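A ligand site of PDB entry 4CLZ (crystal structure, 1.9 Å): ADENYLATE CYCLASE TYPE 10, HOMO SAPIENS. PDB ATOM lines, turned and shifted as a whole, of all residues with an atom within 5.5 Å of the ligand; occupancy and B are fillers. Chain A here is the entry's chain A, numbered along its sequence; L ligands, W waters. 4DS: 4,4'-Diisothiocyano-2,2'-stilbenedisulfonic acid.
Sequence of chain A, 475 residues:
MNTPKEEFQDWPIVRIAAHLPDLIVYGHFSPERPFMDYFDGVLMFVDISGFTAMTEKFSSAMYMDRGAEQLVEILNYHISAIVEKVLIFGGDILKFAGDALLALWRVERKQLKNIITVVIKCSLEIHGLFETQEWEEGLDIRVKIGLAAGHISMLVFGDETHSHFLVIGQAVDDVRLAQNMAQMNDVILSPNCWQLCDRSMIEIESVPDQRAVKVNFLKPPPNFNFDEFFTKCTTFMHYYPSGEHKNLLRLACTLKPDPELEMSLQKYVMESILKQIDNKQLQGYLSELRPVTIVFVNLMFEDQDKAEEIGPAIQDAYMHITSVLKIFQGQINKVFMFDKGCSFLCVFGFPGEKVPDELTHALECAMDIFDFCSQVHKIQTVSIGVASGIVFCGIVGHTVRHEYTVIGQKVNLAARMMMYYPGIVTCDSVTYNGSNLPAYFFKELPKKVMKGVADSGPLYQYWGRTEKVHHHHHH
NE2 of Gln 276 is in hydrogen-bond range of OAD of the ligand, 2.9 Å away. An oxygen (OAA) of the ligand is in salt-bridge range of the guanidinium group (NE) of Arg 15, 3.98 Å away. SBB of the ligand lies close to OD1 of Asn 279, at 3.5 Å. The side-chain amide oxygen of Gln 283 sits close to a nitrogen (NAZ) of the ligand. N of CME 253 lies close to a sulfur (SAU) of the ligand, 3.8 Å away.
The side-chain carboxylate (OD2) of Asp 10 is in salt-bridge range of the guanidinium group (NE) of Arg 15 (2.9 Å). The guanidinium group (NH1) of Arg 15 is in hydrogen-bond range of the side-chain amide oxygen (OD1) of Asn 279 (3.0 Å). The backbone carbonyl oxygen (O) of Ile 277 lies within hydrogen-bond range of the guanidinium group (NH1) of Arg 15. O of Thr 399 sits close to ND1 of His 402. SD of CME 253 is in hydrogen-bond range of N of Arg 250. O of Val 400 is in hydrogen-bond range of NH1 of Arg 250 (2.9 Å). The backbone carbonyl oxygen of Ala 18 sits at hydrogen-bond distance from the backbone NH of His 402 (3.0 Å). The backbone carbonyl oxygen (O) of Ala 17 is in hydrogen-bond range of the guanidinium group (NH1) of Arg 250, 3.0 Å away.
The side-chain carboxylate of Asp 10 lies close to an oxygen (OAW) of the ligand (3.3 Å). A sulfur (SBB) of the ligand sits close to the backbone carbonyl oxygen of Gln 281. SAU of the ligand lies close to O of Val 400. Phe 8 touches the ligand. CG1 of Val 14 touches CAT of the ligand, 3.6 Å away. CB of Ala 18 touches CAQ of the ligand, at 3.7 Å. Arg 250 touches the ligand. CB of Ala 252 touches SAU of the ligand (3.8 Å). Ile 277 touches the ligand (CG1 to OAA, 3.6 Å). Thr 399 touches the ligand (CG2 to OAY, 3.3 Å). Hydrophobic or aromatic side chains within 4 Å of the ligand: Phe 8, Val 14, Ala 18, Ala 252 and Ile 277.
Water W5 lies within hydrogen-bond range of an oxygen (OAC) of the ligand (2.8 Å), a ring nitrogen (NE2) of His 19 (3.0 Å) and the side-chain amide nitrogen of Gln 276 (3.2 Å). Water W1 lies within hydrogen-bond range of O of Arg 15 (2.8 Å), NE2 of His 402 (2.8 Å), OAA of the ligand (2.9 Å) and NE2 of His 19 (3.3 Å). Water W4 lies within hydrogen-bond range of NH2 of Arg 15 (2.7 Å), OD1 of Asn 279 (3.2 Å) and NAZ of the ligand (3.4 Å).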
ATOM      1  N   PHE A   8      12.388  -4.728  -2.161  1.00  0.00           N
ATOM      2  CA  PHE A   8      12.958  -5.966  -1.676  1.00  0.00           C
ATOM      3  C   PHE A   8      11.801  -6.914  -1.332  1.00  0.00           C
ATOM      4  O   PHE A   8      10.869  -6.525  -0.621  1.00  0.00           O
ATOM      5  CB  PHE A   8      13.869  -5.744  -0.471  1.00  0.00           C
ATOM      6  CG  PHE A   8      14.213  -7.010   0.228  1.00  0.00           C
ATOM      7  CD1 PHE A   8      15.019  -7.977  -0.410  1.00  0.00           C
ATOM      8  CD2 PHE A   8      13.643  -7.303   1.472  1.00  0.00           C
ATOM      9  CE1 PHE A   8      15.289  -9.200   0.236  1.00  0.00           C
ATOM     10  CE2 PHE A   8      13.936  -8.517   2.113  1.00  0.00           C
ATOM     11  CZ  PHE A   8      14.738  -9.461   1.482  1.00  0.00           C
ATOM     12  N   ASP A  10      10.723 -10.392   0.452  1.00  0.00           N
ATOM     13  CA  ASP A  10      11.022 -11.298   1.480  1.00  0.00           C
ATOM     14  C   ASP A  10      10.291 -12.645   1.253  1.00  0.00           C
ATOM     15  O   ASP A  10       9.589 -13.118   2.186  1.00  0.00           O
ATOM     16  CB  ASP A  10      10.471 -10.592   2.717  1.00  0.00           C
ATOM     17  CG  ASP A  10      10.946 -11.175   3.921  1.00  0.00           C
ATOM     18  OD1 ASP A  10      12.048 -11.775   3.848  1.00  0.00           O
ATOM     19  OD2 ASP A  10      10.224 -11.066   4.909  1.00  0.00           O
ATOM     20  N   VAL A  14      13.742 -16.779   0.376  1.00  0.00           N
ATOM     21  CA  VAL A  14      14.741 -15.888   0.938  1.00  0.00           C
ATOM     22  C   VAL A  14      14.828 -15.989   2.464  1.00  0.00           C
ATOM     23  O   VAL A  14      15.902 -15.978   3.044  1.00  0.00           O
ATOM     24  CB  VAL A  14      14.416 -14.424   0.556  1.00  0.00           C
ATOM     25  CG1 VAL A  14      15.313 -13.427   1.245  1.00  0.00           C
ATOM     26  CG2 VAL A  14      14.477 -14.217  -0.976  1.00  0.00           C
ATOM     27  N   ARG A  15      13.659 -16.059   3.106  1.00  0.00           N
ATOM     28  CA  ARG A  15      13.627 -16.287   4.565  1.00  0.00           C
ATOM     29  C   ARG A  15      14.342 -17.585   4.965  1.00  0.00           C
ATOM     30  O   ARG A  15      15.097 -17.560   5.928  1.00  0.00           O
ATOM     31  CB  ARG A  15      12.212 -16.266   5.051  1.00  0.00           C
ATOM     32  CG  ARG A  15      11.465 -14.956   4.839  1.00  0.00           C
ATOM     33  CD  ARG A  15       9.997 -15.067   5.352  1.00  0.00           C
ATOM     34  NE  ARG A  15       9.366 -13.779   5.406  1.00  0.00           N
ATOM     35  CZ  ARG A  15       8.276 -13.506   6.120  1.00  0.00           C
ATOM     36  NH1 ARG A  15       7.713 -14.456   6.800  1.00  0.00           N
ATOM     37  NH2 ARG A  15       7.783 -12.252   6.170  1.00  0.00           N
ATOM     38  N   ALA A  17      16.745 -18.981   3.122  1.00  0.00           N
ATOM     39  CA  ALA A  17      18.171 -18.766   2.846  1.00  0.00           C
ATOM     40  C   ALA A  17      18.919 -18.004   3.917  1.00  0.00           C
ATOM     41  O   ALA A  17      20.131 -18.204   4.073  1.00  0.00           O
ATOM     42  CB  ALA A  17      18.342 -18.094   1.511  1.00  0.00           C
ATOM     43  N   ALA A  18      18.236 -17.153   4.675  1.00  0.00           N
ATOM     44  CA  ALA A  18      18.909 -16.467   5.804  1.00  0.00           C
ATOM     45  C   ALA A  18      19.456 -17.434   6.842  1.00  0.00           C
ATOM     46  O   ALA A  18      20.463 -17.162   7.478  1.00  0.00           O
ATOM     47  CB  ALA A  18      17.949 -15.490   6.475  1.00  0.00           C
ATOM     48  N   HIS A  19      18.879 -18.624   6.934  1.00  0.00           N
ATOM     49  CA  HIS A  19      19.365 -19.680   7.879  1.00  0.00           C
ATOM     50  C   HIS A  19      20.528 -20.487   7.405  1.00  0.00           C
ATOM     51  O   HIS A  19      21.028 -21.384   8.154  1.00  0.00           O
ATOM     52  CB  HIS A  19      18.232 -20.606   8.275  1.00  0.00           C
ATOM     53  CG  HIS A  19      17.214 -19.921   9.103  1.00  0.00           C
ATOM     54  ND1 HIS A  19      17.161 -20.031  10.487  1.00  0.00           N
ATOM     55  CD2 HIS A  19      16.229 -19.088   8.743  1.00  0.00           C
ATOM     56  CE1 HIS A  19      16.186 -19.263  10.941  1.00  0.00           C
ATOM     57  NE2 HIS A  19      15.620 -18.659   9.899  1.00  0.00           N
ATOM     58  N   ARG A 250      23.932  -9.730   1.066  1.00  0.00           N
ATOM     59  CA  ARG A 250      24.027 -11.048   0.453  1.00  0.00           C
ATOM     60  C   ARG A 250      23.292 -11.124  -0.850  1.00  0.00           C
ATOM     61  O   ARG A 250      22.174 -10.606  -0.985  1.00  0.00           O
ATOM     62  CB  ARG A 250      23.386 -12.150   1.331  1.00  0.00           C
ATOM     63  CG  ARG A 250      23.903 -12.244   2.717  1.00  0.00           C
ATOM     64  CD  ARG A 250      23.276 -13.385   3.487  1.00  0.00           C
ATOM     65  NE  ARG A 250      23.696 -14.712   2.966  1.00  0.00           N
ATOM     66  CZ  ARG A 250      23.093 -15.857   3.256  1.00  0.00           C
ATOM     67  NH1 ARG A 250      22.049 -15.868   4.107  1.00  0.00           N
ATOM     68  NH2 ARG A 250      23.564 -16.971   2.768  1.00  0.00           N
ATOM     69  N   ALA A 252      21.974 -13.820  -1.724  1.00  0.00           N
ATOM     70  CA  ALA A 252      20.816 -14.638  -1.386  1.00  0.00           C
ATOM     71  C   ALA A 252      19.553 -13.808  -1.125  1.00  0.00           C
ATOM     72  O   ALA A 252      18.428 -14.324  -1.250  1.00  0.00           O
ATOM     73  CB  ALA A 252      21.162 -15.473  -0.153  1.00  0.00           C
ATOM     74  N   CME A 253      19.724 -12.531  -0.791  1.00  0.00           N
ATOM     75  CA  CME A 253      18.566 -11.622  -0.685  1.00  0.00           C
ATOM     76  CB  CME A 253      18.993 -10.192  -0.255  1.00  0.00           C
ATOM     77  SG  CME A 253      19.627 -10.251   1.450  1.00  0.00           S
ATOM     78  SD  CME A 253      20.530  -8.494   1.642  1.00  0.00           S
ATOM     79  CE  CME A 253      19.310  -7.259   2.037  1.00  0.00           C
ATOM     80  CZ  CME A 253      20.029  -6.314   3.030  1.00  0.00           C
ATOM     81  OH  CME A 253      21.387  -5.920   2.653  1.00  0.00           O
ATOM     82  C   CME A 253      17.820 -11.521  -2.038  1.00  0.00           C
ATOM     83  O   CME A 253      16.638 -11.164  -2.043  1.00  0.00           O
ATOM     84  N   ILE A 273      10.922 -23.504  12.867  1.00  0.00           N
ATOM     85  CA  ILE A 273      11.412 -22.291  12.221  1.00  0.00           C
ATOM     86  C   ILE A 273      10.637 -22.004  10.924  1.00  0.00           C
ATOM     87  O   ILE A 273      10.269 -20.876  10.604  1.00  0.00           O
ATOM     88  CB  ILE A 273      12.909 -22.411  11.949  1.00  0.00           C
ATOM     89  CG1 ILE A 273      13.744 -22.337  13.250  1.00  0.00           C
ATOM     90  CG2 ILE A 273      13.351 -21.359  10.968  1.00  0.00           C
ATOM     91  CD1 ILE A 273      13.836 -20.972  13.802  1.00  0.00           C
ATOM     92  N   GLN A 276       7.364 -20.331  11.570  1.00  0.00           N
ATOM     93  CA  GLN A 276       7.559 -18.877  11.684  1.00  0.00           C
ATOM     94  C   GLN A 276       7.710 -18.193  10.345  1.00  0.00           C
ATOM     95  O   GLN A 276       7.108 -17.151  10.067  1.00  0.00           O
ATOM     96  CB  GLN A 276       8.719 -18.579  12.644  1.00  0.00           C
ATOM     97  CG  GLN A 276       8.908 -17.102  12.853  1.00  0.00           C
ATOM     98  CD  GLN A 276      10.186 -16.817  13.668  1.00  0.00           C
ATOM     99  OE1 GLN A 276      10.352 -17.336  14.789  1.00  0.00           O
ATOM    100  NE2 GLN A 276      11.132 -16.125  13.050  1.00  0.00           N
ATOM    101  N   ILE A 277       8.563 -18.782   9.516  1.00  0.00           N
ATOM    102  CA  ILE A 277       8.810 -18.312   8.150  1.00  0.00           C
ATOM    103  C   ILE A 277       7.527 -18.198   7.379  1.00  0.00           C
ATOM    104  O   ILE A 277       7.333 -17.225   6.570  1.00  0.00           O
ATOM    105  CB  ILE A 277       9.879 -19.186   7.449  1.00  0.00           C
ATOM    106  CG1 ILE A 277      11.274 -18.850   8.051  1.00  0.00           C
ATOM    107  CG2 ILE A 277       9.763 -19.008   5.954  1.00  0.00           C
ATOM    108  CD1 ILE A 277      12.416 -19.663   7.530  1.00  0.00           C
ATOM    109  N   ASN A 279       4.656 -17.503   8.434  1.00  0.00           N
ATOM    110  CA  ASN A 279       3.710 -16.639   9.145  1.00  0.00           C
ATOM    111  C   ASN A 279       2.589 -17.380   9.779  1.00  0.00           C
ATOM    112  O   ASN A 279       1.452 -16.902   9.854  1.00  0.00           O
ATOM    113  CB  ASN A 279       3.173 -15.604   8.201  1.00  0.00           C
ATOM    114  CG  ASN A 279       4.225 -14.684   7.650  1.00  0.00           C
ATOM    115  OD1 ASN A 279       5.151 -14.259   8.325  1.00  0.00           O
ATOM    116  ND2 ASN A 279       4.066 -14.353   6.414  1.00  0.00           N
ATOM    117  N   LYS A 280       2.896 -18.546  10.309  1.00  0.00           N
ATOM    118  CA  LYS A 280       1.931 -19.378  10.997  1.00  0.00           C
ATOM    119  C   LYS A 280       2.216 -19.469  12.517  1.00  0.00           C
ATOM    120  O   LYS A 280       1.540 -20.156  13.195  1.00  0.00           O
ATOM    121  CB  LYS A 280       1.845 -20.761  10.336  1.00  0.00           C
ATOM    122  CG  LYS A 280       1.036 -20.758   9.006  1.00  0.00           C
ATOM    123  CD  LYS A 280       0.926 -22.132   8.333  1.00  0.00           C
ATOM    124  CE  LYS A 280      -0.100 -22.129   7.152  1.00  0.00           C
ATOM    125  NZ  LYS A 280       0.235 -21.354   5.876  1.00  0.00           N
ATOM    126  N   GLN A 281       3.220 -18.729  13.027  1.00  0.00           N
ATOM    127  CA  GLN A 281       3.565 -18.685  14.440  1.00  0.00           C
ATOM    128  C   GLN A 281       4.181 -17.313  14.681  1.00  0.00           C
ATOM    129  O   GLN A 281       4.880 -16.757  13.847  1.00  0.00           O
ATOM    130  CB  GLN A 281       4.596 -19.790  14.711  1.00  0.00           C
ATOM    131  CG  GLN A 281       5.189 -19.995  16.048  1.00  0.00           C
ATOM    132  CD  GLN A 281       6.121 -21.252  15.928  1.00  0.00           C
ATOM    133  OE1 GLN A 281       5.605 -22.342  15.888  1.00  0.00           O
ATOM    134  NE2 GLN A 281       7.435 -21.073  15.687  1.00  0.00           N
ATOM    135  N   LEU A 282       3.886 -16.752  15.816  1.00  0.00           N
ATOM    136  CA  LEU A 282       4.468 -15.405  16.124  1.00  0.00           C
ATOM    137  C   LEU A 282       5.970 -15.447  16.229  1.00  0.00           C
ATOM    138  O   LEU A 282       6.528 -16.460  16.648  1.00  0.00           O
ATOM    139  CB  LEU A 282       3.875 -14.965  17.438  1.00  0.00           C
ATOM    140  CG  LEU A 282       2.366 -14.687  17.433  1.00  0.00           C
ATOM    141  CD1 LEU A 282       1.710 -14.644  18.806  1.00  0.00           C
ATOM    142  CD2 LEU A 282       2.121 -13.378  16.731  1.00  0.00           C
ATOM    143  N   GLN A 283       6.625 -14.390  15.787  1.00  0.00           N
ATOM    144  CA  GLN A 283       8.093 -14.323  15.755  1.00  0.00           C
ATOM    145  C   GLN A 283       8.694 -14.415  17.074  1.00  0.00           C
ATOM    146  O   GLN A 283       9.826 -14.829  17.204  1.00  0.00           O
ATOM    147  CB  GLN A 283       8.583 -13.047  15.187  1.00  0.00           C
ATOM    148  CG  GLN A 283       8.568 -12.937  13.723  1.00  0.00           C
ATOM    149  CD  GLN A 283       9.302 -11.691  13.292  1.00  0.00           C
ATOM    150  OE1 GLN A 283       8.670 -10.686  12.996  1.00  0.00           O
ATOM    151  NE2 GLN A 283      10.626 -11.763  13.249  1.00  0.00           N
ATOM    152  N   THR A 399      19.665 -10.049  10.575  1.00  0.00           N
ATOM    153  CA  THR A 399      18.472 -10.179   9.717  1.00  0.00           C
ATOM    154  C   THR A 399      18.743 -11.055   8.503  1.00  0.00           C
ATOM    155  O   THR A 399      17.931 -11.870   8.155  1.00  0.00           O
ATOM    156  CB  THR A 399      18.059  -8.808   9.211  1.00  0.00           C
ATOM    157  OG1 THR A 399      17.793  -8.040  10.370  1.00  0.00           O
ATOM    158  CG2 THR A 399      16.814  -8.843   8.293  1.00  0.00           C
ATOM    159  N   VAL A 400      19.889 -10.907   7.863  1.00  0.00           N
ATOM    160  CA  VAL A 400      20.138 -11.650   6.608  1.00  0.00           C
ATOM    161  C   VAL A 400      20.888 -12.967   6.759  1.00  0.00           C
ATOM    162  O   VAL A 400      20.973 -13.699   5.789  1.00  0.00           O
ATOM    163  CB  VAL A 400      20.879 -10.762   5.577  1.00  0.00           C
ATOM    164  CG1 VAL A 400      20.135  -9.439   5.384  1.00  0.00           C
ATOM    165  CG2 VAL A 400      22.329 -10.634   5.954  1.00  0.00           C
ATOM    166  N   HIS A 402      21.249 -15.735  10.051  1.00  0.00           N
ATOM    167  CA  HIS A 402      20.913 -16.106  11.418  1.00  0.00           C
ATOM    168  C   HIS A 402      20.553 -17.572  11.560  1.00  0.00           C
ATOM    169  O   HIS A 402      20.258 -18.220  10.595  1.00  0.00           O
ATOM    170  CB  HIS A 402      19.811 -15.258  12.000  1.00  0.00           C
ATOM    171  CG  HIS A 402      18.566 -15.198  11.199  1.00  0.00           C
ATOM    172  ND1 HIS A 402      18.092 -14.022  10.709  1.00  0.00           N
ATOM    173  CD2 HIS A 402      17.780 -16.151  10.632  1.00  0.00           C
ATOM    174  CE1 HIS A 402      16.991 -14.222   9.999  1.00  0.00           C
ATOM    175  NE2 HIS A 402      16.787 -15.498   9.931  1.00  0.00           N
HETATM  176  OAA 4DS L   1      11.877 -15.324   8.077  1.00  0.00           O
HETATM  177  SAB 4DS L   1      11.409 -14.860   9.390  1.00  0.00           S
HETATM  178  OAC 4DS L   1      12.583 -14.442  10.142  1.00  0.00           O
HETATM  179  OAD 4DS L   1      10.646 -15.868  10.179  1.00  0.00           O
HETATM  180  CAE 4DS L   1      10.462 -13.387   9.227  1.00  0.00           C
HETATM  181  CAF 4DS L   1       9.185 -13.391   9.867  1.00  0.00           C
HETATM  182  CAG 4DS L   1       8.391 -12.235   9.772  1.00  0.00           C
HETATM  183  CAH 4DS L   1       8.898 -11.130   9.064  1.00  0.00           C
HETATM  184  CAI 4DS L   1      10.160 -11.146   8.441  1.00  0.00           C
HETATM  185  CAJ 4DS L   1      10.976 -12.294   8.531  1.00  0.00           C
HETATM  186  CAK 4DS L   1      12.269 -12.361   7.892  1.00  0.00           C
HETATM  187  CAL 4DS L   1      12.697 -11.464   6.946  1.00  0.00           C
HETATM  188  CAM 4DS L   1      13.915 -11.527   6.242  1.00  0.00           C
HETATM  189  CAN 4DS L   1      14.570 -10.426   5.651  1.00  0.00           C
HETATM  190  CAO 4DS L   1      15.748 -10.566   4.925  1.00  0.00           C
HETATM  191  CAP 4DS L   1      16.267 -11.851   4.732  1.00  0.00           C
HETATM  192  CAQ 4DS L   1      15.564 -12.918   5.245  1.00  0.00           C
HETATM  193  CAR 4DS L   1      14.415 -12.776   5.965  1.00  0.00           C
HETATM  194  NAS 4DS L   1      17.359 -12.007   4.016  1.00  0.00           N
HETATM  195  CAT 4DS L   1      18.099 -12.857   3.443  1.00  0.00           C
HETATM  196  SAU 4DS L   1      19.116 -13.918   2.665  1.00  0.00           S
HETATM  197  SAV 4DS L   1      13.860  -8.794   5.926  1.00  0.00           S
HETATM  198  OAW 4DS L   1      12.557  -8.723   5.231  1.00  0.00           O
HETATM  199  OAX 4DS L   1      14.868  -7.880   5.491  1.00  0.00           O
HETATM  200  OAY 4DS L   1      13.596  -8.798   7.409  1.00  0.00           O
HETATM  201  NAZ 4DS L   1       7.166 -12.215  10.359  1.00  0.00           N
HETATM  202  CBA 4DS L   1       6.745 -13.281  10.937  1.00  0.00           C
HETATM  203  SBB 4DS L   1       6.158 -14.699  11.700  1.00  0.00           S
HETATM  204  O   HOH W   1      14.674 -16.039   8.181  1.00  0.00           O
HETATM  205  O   HOH W   2      17.203  -6.703   4.913  1.00  0.00           O
HETATM  206  O   HOH W   3      13.986  -5.200   4.831  1.00  0.00           O
HETATM  207  O   HOH W   4       5.649 -11.249   7.431  1.00  0.00           O
HETATM  208  O   HOH W   5      13.446 -16.938  10.938  1.00  0.00           O
